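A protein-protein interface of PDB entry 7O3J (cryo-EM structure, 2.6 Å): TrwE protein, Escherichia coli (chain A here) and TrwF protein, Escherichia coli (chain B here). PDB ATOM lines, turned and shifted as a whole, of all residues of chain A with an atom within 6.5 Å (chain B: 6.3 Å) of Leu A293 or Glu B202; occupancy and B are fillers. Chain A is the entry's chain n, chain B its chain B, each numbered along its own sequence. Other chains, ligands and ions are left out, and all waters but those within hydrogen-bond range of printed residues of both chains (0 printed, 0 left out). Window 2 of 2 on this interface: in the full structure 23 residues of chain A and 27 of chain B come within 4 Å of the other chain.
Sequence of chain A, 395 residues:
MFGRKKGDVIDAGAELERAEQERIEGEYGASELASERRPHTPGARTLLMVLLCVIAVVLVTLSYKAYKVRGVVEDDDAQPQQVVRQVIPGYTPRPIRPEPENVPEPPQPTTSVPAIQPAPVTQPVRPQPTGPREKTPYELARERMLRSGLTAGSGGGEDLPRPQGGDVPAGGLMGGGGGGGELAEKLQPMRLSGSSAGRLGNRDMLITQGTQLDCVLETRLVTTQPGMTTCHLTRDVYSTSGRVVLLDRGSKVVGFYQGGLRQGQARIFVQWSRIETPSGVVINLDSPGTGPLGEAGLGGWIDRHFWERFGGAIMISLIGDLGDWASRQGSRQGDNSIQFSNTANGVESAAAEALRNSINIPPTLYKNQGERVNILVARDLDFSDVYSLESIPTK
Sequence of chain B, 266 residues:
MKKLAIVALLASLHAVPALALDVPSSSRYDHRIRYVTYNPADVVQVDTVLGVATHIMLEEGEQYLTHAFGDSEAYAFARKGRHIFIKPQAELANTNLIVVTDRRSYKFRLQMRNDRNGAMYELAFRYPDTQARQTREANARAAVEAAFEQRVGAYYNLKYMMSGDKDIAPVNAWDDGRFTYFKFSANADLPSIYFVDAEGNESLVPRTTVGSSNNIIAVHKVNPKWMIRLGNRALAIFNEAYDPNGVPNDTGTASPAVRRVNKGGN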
ATOM      1  N   THR A 290      11.329  32.167  13.394  1.00  0.00           N
ATOM      2  CA  THR A 290      10.765  31.109  12.577  1.00  0.00           C
ATOM      3  C   THR A 290      10.146  30.053  13.483  1.00  0.00           C
ATOM      4  O   THR A 290      10.133  30.183  14.705  1.00  0.00           O
ATOM      5  CB  THR A 290      11.837  30.499  11.665  1.00  0.00           C
ATOM      6  OG1 THR A 290      12.947  30.060  12.452  1.00  0.00           O
ATOM      7  CG2 THR A 290      12.334  31.519  10.663  1.00  0.00           C
ATOM      8  N   GLY A 291       9.616  29.004  12.873  1.00  0.00           N
ATOM      9  CA  GLY A 291       9.121  27.878  13.620  1.00  0.00           C
ATOM     10  C   GLY A 291      10.222  26.904  13.944  1.00  0.00           C
ATOM     11  O   GLY A 291      11.400  27.129  13.668  1.00  0.00           O
ATOM     12  N   PRO A 292       9.839  25.784  14.557  1.00  0.00           N
ATOM     13  CA  PRO A 292      10.842  24.771  14.912  1.00  0.00           C
ATOM     14  C   PRO A 292      11.584  24.201  13.719  1.00  0.00           C
ATOM     15  O   PRO A 292      12.732  23.771  13.865  1.00  0.00           O
ATOM     16  CB  PRO A 292      10.014  23.697  15.625  1.00  0.00           C
ATOM     17  CG  PRO A 292       8.786  24.380  16.043  1.00  0.00           C
ATOM     18  CD  PRO A 292       8.497  25.404  15.010  1.00  0.00           C
ATOM     19  N   LEU A 293      10.964  24.178  12.540  1.00  0.00           N
ATOM     20  CA  LEU A 293      11.599  23.667  11.335  1.00  0.00           C
ATOM     21  C   LEU A 293      11.957  24.772  10.356  1.00  0.00           C
ATOM     22  O   LEU A 293      12.159  24.503   9.171  1.00  0.00           O
ATOM     23  CB  LEU A 293      10.703  22.636  10.655  1.00  0.00           C
ATOM     24  CG  LEU A 293      10.854  21.213  11.171  1.00  0.00           C
ATOM     25  CD1 LEU A 293       9.688  20.395  10.703  1.00  0.00           C
ATOM     26  CD2 LEU A 293      12.153  20.618  10.700  1.00  0.00           C
ATOM     27  N   GLY A 294      12.035  26.008  10.823  1.00  0.00           N
ATOM     28  CA  GLY A 294      12.534  27.093  10.014  1.00  0.00           C
ATOM     29  C   GLY A 294      11.528  27.772   9.122  1.00  0.00           C
ATOM     30  O   GLY A 294      11.922  28.619   8.315  1.00  0.00           O
ATOM     31  N   GLU A 295      10.250  27.433   9.224  1.00  0.00           N
ATOM     32  CA  GLU A 295       9.245  28.121   8.431  1.00  0.00           C
ATOM     33  C   GLU A 295       8.996  29.520   8.975  1.00  0.00           C
ATOM     34  O   GLU A 295       8.961  29.737  10.185  1.00  0.00           O
ATOM     35  CB  GLU A 295       7.966  27.291   8.372  1.00  0.00           C
ATOM     36  CG  GLU A 295       7.292  27.083   9.683  1.00  0.00           C
ATOM     37  CD  GLU A 295       7.708  25.781  10.331  1.00  0.00           C
ATOM     38  OE1 GLU A 295       8.911  25.602  10.574  1.00  0.00           O
ATOM     39  OE2 GLU A 295       6.837  24.934  10.600  1.00  0.00           O
ATOM     40  N   ASN A 374      12.826  28.947  16.465  1.00  0.00           N
ATOM     41  CA  ASN A 374      14.171  29.184  15.962  1.00  0.00           C
ATOM     42  C   ASN A 374      14.368  30.648  15.620  1.00  0.00           C
ATOM     43  O   ASN A 374      13.425  31.357  15.262  1.00  0.00           O
ATOM     44  CB  ASN A 374      14.500  28.355  14.716  1.00  0.00           C
ATOM     45  CG  ASN A 374      14.653  26.889  15.009  1.00  0.00           C
ATOM     46  OD1 ASN A 374      15.250  26.500  16.008  1.00  0.00           O
ATOM     47  ND2 ASN A 374      14.123  26.058  14.130  1.00  0.00           N
ATOM     48  N   TYR B 194      17.992  15.984  11.126  1.00  0.00           N
ATOM     49  CA  TYR B 194      17.026  16.678  11.960  1.00  0.00           C
ATOM     50  C   TYR B 194      16.975  16.074  13.349  1.00  0.00           C
ATOM     51  O   TYR B 194      17.227  14.887  13.547  1.00  0.00           O
ATOM     52  CB  TYR B 194      15.634  16.656  11.337  1.00  0.00           C
ATOM     53  CG  TYR B 194      15.603  17.428  10.061  1.00  0.00           C
ATOM     54  CD1 TYR B 194      15.555  18.804  10.077  1.00  0.00           C
ATOM     55  CD2 TYR B 194      15.671  16.790   8.841  1.00  0.00           C
ATOM     56  CE1 TYR B 194      15.557  19.519   8.925  1.00  0.00           C
ATOM     57  CE2 TYR B 194      15.672  17.501   7.680  1.00  0.00           C
ATOM     58  CZ  TYR B 194      15.616  18.866   7.731  1.00  0.00           C
ATOM     59  OH  TYR B 194      15.612  19.597   6.578  1.00  0.00           O
ATOM     60  N   PHE B 195      16.629  16.921  14.305  1.00  0.00           N
ATOM     61  CA  PHE B 195      16.566  16.571  15.713  1.00  0.00           C
ATOM     62  C   PHE B 195      15.143  16.145  16.041  1.00  0.00           C
ATOM     63  O   PHE B 195      14.194  16.877  15.757  1.00  0.00           O
ATOM     64  CB  PHE B 195      17.005  17.787  16.535  1.00  0.00           C
ATOM     65  CG  PHE B 195      16.691  17.712  17.992  1.00  0.00           C
ATOM     66  CD1 PHE B 195      15.470  18.134  18.478  1.00  0.00           C
ATOM     67  CD2 PHE B 195      17.641  17.280  18.887  1.00  0.00           C
ATOM     68  CE1 PHE B 195      15.192  18.082  19.814  1.00  0.00           C
ATOM     69  CE2 PHE B 195      17.366  17.234  20.228  1.00  0.00           C
ATOM     70  CZ  PHE B 195      16.140  17.632  20.690  1.00  0.00           C
ATOM     71  N   VAL B 196      14.992  14.961  16.622  1.00  0.00           N
ATOM     72  CA  VAL B 196      13.684  14.400  16.940  1.00  0.00           C
ATOM     73  C   VAL B 196      13.497  14.424  18.448  1.00  0.00           C
ATOM     74  O   VAL B 196      14.345  13.920  19.191  1.00  0.00           O
ATOM     75  CB  VAL B 196      13.534  12.973  16.389  1.00  0.00           C
ATOM     76  CG1 VAL B 196      12.250  12.367  16.870  1.00  0.00           C
ATOM     77  CG2 VAL B 196      13.553  12.995  14.889  1.00  0.00           C
ATOM     78  N   ASP B 197      12.391  15.004  18.897  1.00  0.00           N
ATOM     79  CA  ASP B 197      12.097  15.088  20.317  1.00  0.00           C
ATOM     80  C   ASP B 197      11.259  13.886  20.755  1.00  0.00           C
ATOM     81  O   ASP B 197      11.011  12.957  19.983  1.00  0.00           O
ATOM     82  CB  ASP B 197      11.437  16.427  20.637  1.00  0.00           C
ATOM     83  CG  ASP B 197      10.014  16.533  20.123  1.00  0.00           C
ATOM     84  OD1 ASP B 197       9.388  17.584  20.361  1.00  0.00           O
ATOM     85  OD2 ASP B 197       9.522  15.605  19.454  1.00  0.00           O
ATOM     86  N   GLY B 200       8.102  13.169  18.818  1.00  0.00           N
ATOM     87  CA  GLY B 200       8.303  12.859  17.423  1.00  0.00           C
ATOM     88  C   GLY B 200       8.391  14.052  16.501  1.00  0.00           C
ATOM     89  O   GLY B 200       8.439  13.864  15.283  1.00  0.00           O
ATOM     90  N   ASN B 201       8.410  15.265  17.037  1.00  0.00           N
ATOM     91  CA  ASN B 201       8.526  16.454  16.209  1.00  0.00           C
ATOM     92  C   ASN B 201       9.976  16.705  15.833  1.00  0.00           C
ATOM     93  O   ASN B 201      10.883  16.565  16.657  1.00  0.00           O
ATOM     94  CB  ASN B 201       7.963  17.670  16.936  1.00  0.00           C
ATOM     95  CG  ASN B 201       6.652  17.383  17.610  1.00  0.00           C
ATOM     96  OD1 ASN B 201       5.657  17.090  16.952  1.00  0.00           O
ATOM     97  ND2 ASN B 201       6.639  17.453  18.931  1.00  0.00           N
ATOM     98  N   GLU B 202      10.187  17.083  14.581  1.00  0.00           N
ATOM     99  CA  GLU B 202      11.512  17.336  14.049  1.00  0.00           C
ATOM    100  C   GLU B 202      11.852  18.809  14.208  1.00  0.00           C
ATOM    101  O   GLU B 202      10.980  19.675  14.130  1.00  0.00           O
ATOM    102  CB  GLU B 202      11.553  16.959  12.575  1.00  0.00           C
ATOM    103  CG  GLU B 202      11.394  15.490  12.316  1.00  0.00           C
ATOM    104  CD  GLU B 202      11.416  15.182  10.844  1.00  0.00           C
ATOM    105  OE1 GLU B 202      11.440  16.134  10.041  1.00  0.00           O
ATOM    106  OE2 GLU B 202      11.346  13.994  10.483  1.00  0.00           O
ATOM    107  N   SER B 203      13.129  19.094  14.431  1.00  0.00           N
ATOM    108  CA  SER B 203      13.556  20.481  14.498  1.00  0.00           C
ATOM    109  C   SER B 203      14.985  20.593  14.003  1.00  0.00           C
ATOM    110  O   SER B 203      15.747  19.627  14.014  1.00  0.00           O
ATOM    111  CB  SER B 203      13.428  21.047  15.913  1.00  0.00           C
ATOM    112  OG  SER B 203      14.251  20.350  16.825  1.00  0.00           O
ATOM    113  N   LEU B 204      15.335  21.795  13.563  1.00  0.00           N
ATOM    114  CA  LEU B 204      16.666  22.043  13.037  1.00  0.00           C
ATOM    115  C   LEU B 204      17.705  21.977  14.141  1.00  0.00           C
ATOM    116  O   LEU B 204      17.454  22.376  15.279  1.00  0.00           O
ATOM    117  CB  LEU B 204      16.727  23.410  12.363  1.00  0.00           C
ATOM    118  CG  LEU B 204      15.595  23.776  11.419  1.00  0.00           C
ATOM    119  CD1 LEU B 204      15.585  25.259  11.199  1.00  0.00           C
ATOM    120  CD2 LEU B 204      15.763  23.052  10.114  1.00  0.00           C
ATOM    121  N   MET B 227      16.811  12.136  12.616  1.00  0.00           N
ATOM    122  CA  MET B 227      16.098  11.932  11.364  1.00  0.00           C
ATOM    123  C   MET B 227      16.969  12.408  10.216  1.00  0.00           C
ATOM    124  O   MET B 227      17.500  13.517  10.258  1.00  0.00           O
ATOM    125  CB  MET B 227      14.775  12.686  11.354  1.00  0.00           C
ATOM    126  CG  MET B 227      13.925  12.421  10.143  1.00  0.00           C
ATOM    127  SD  MET B 227      13.636  10.670   9.907  1.00  0.00           S
ATOM    128  CE  MET B 227      12.261  10.447  11.017  1.00  0.00           C
ATOM    129  N   ARG B 229      17.013  13.015   6.079  1.00  0.00           N
ATOM    130  CA  ARG B 229      16.132  13.203   4.938  1.00  0.00           C
ATOM    131  C   ARG B 229      16.930  13.693   3.744  1.00  0.00           C
ATOM    132  O   ARG B 229      17.763  14.592   3.880  1.00  0.00           O
ATOM    133  CB  ARG B 229      15.026  14.204   5.253  1.00  0.00           C
ATOM    134  CG  ARG B 229      14.142  13.813   6.400  1.00  0.00           C
ATOM    135  CD  ARG B 229      12.911  14.675   6.443  1.00  0.00           C
ATOM    136  NE  ARG B 229      11.962  14.203   7.437  1.00  0.00           N
ATOM    137  CZ  ARG B 229      11.085  13.235   7.221  1.00  0.00           C
ATOM    138  NH1 ARG B 229      11.038  12.637   6.045  1.00  0.00           N
ATOM    139  NH2 ARG B 229      10.256  12.865   8.182  1.00  0.00           N
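CA of Ser B203 touches O of Pro A292, at 3.5 Å. Leu A293 touches Tyr B194. Leu A293 touches Glu B202. Leu B204 touches Leu A293. N of Gly A294 touches CD1 of Leu B204, 3.6 Å away. Asn A374 touches Leu B204 (ND2 to CD1, 3.4 Å).
Printed residues of chain B within 4 Å of Leu A293: Tyr B194, Glu B202 and Leu B204. Of the printed residues of chain B, Pro A292 touches Ser B203 (3.5 Å) and Leu B204 (3.3 Å). Of the printed residues of chain A, Leu B204 touches Pro A292 (3.3 Å), Leu A293 (3.8 Å), Gly A294 (3.6 Å) and Asn A374 (3.4 Å). Of the printed residues of chain B, Gly A294 touches Leu B204 (3.6 Å). The nearest printed residue of chain B that does not touch Pro A292 is Glu B202 (4.4 Å).
Of the 11 printed residues of chain B, 4 touch a printed residue of chain A. Printed residues of chain B that touch a printed residue of chain A: Tyr B194, Glu B202, Ser B203 and Leu B204. Of the 7 printed residues of chain A, 4 touch a printed residue of chain B. Among the printed residues, 7 pairs touch across the chains. Among the printed residues, no Asp or Glu carboxylate lies within 4 Å of a Lys or Arg side-chain nitrogen of the other chain.
O of Phe B195 sits at hydrogen-bond distance from N of Ser B203 (2.8 Å). The backbone NH (N) of Leu A293 lies close to the side-chain carboxylate (OE1) of Glu A295, 3.2 Å away. The backbone NH of Thr A290 is in hydrogen-bond range of the backbone carbonyl oxygen of Asn A374 (2.9 Å). The backbone NH (N) of Tyr B194 sits at hydrogen-bond distance from the backbone carbonyl oxygen (O) of Met B227 (2.7 Å). The backbone carbonyl oxygen of Gly A291 sits at hydrogen-bond distance from the side-chain amide nitrogen of Asn A374, at 3.0 Å. The side-chain carboxylate (OE2) of Glu B202 is in salt-bridge range of the guanidinium group (NH2) of Arg B229, 2.8 Å away.
The backbone carbonyl oxygen of Pro A292 lies within hydrogen-bond range of the backbone NH of Leu B204 (3.3 Å).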
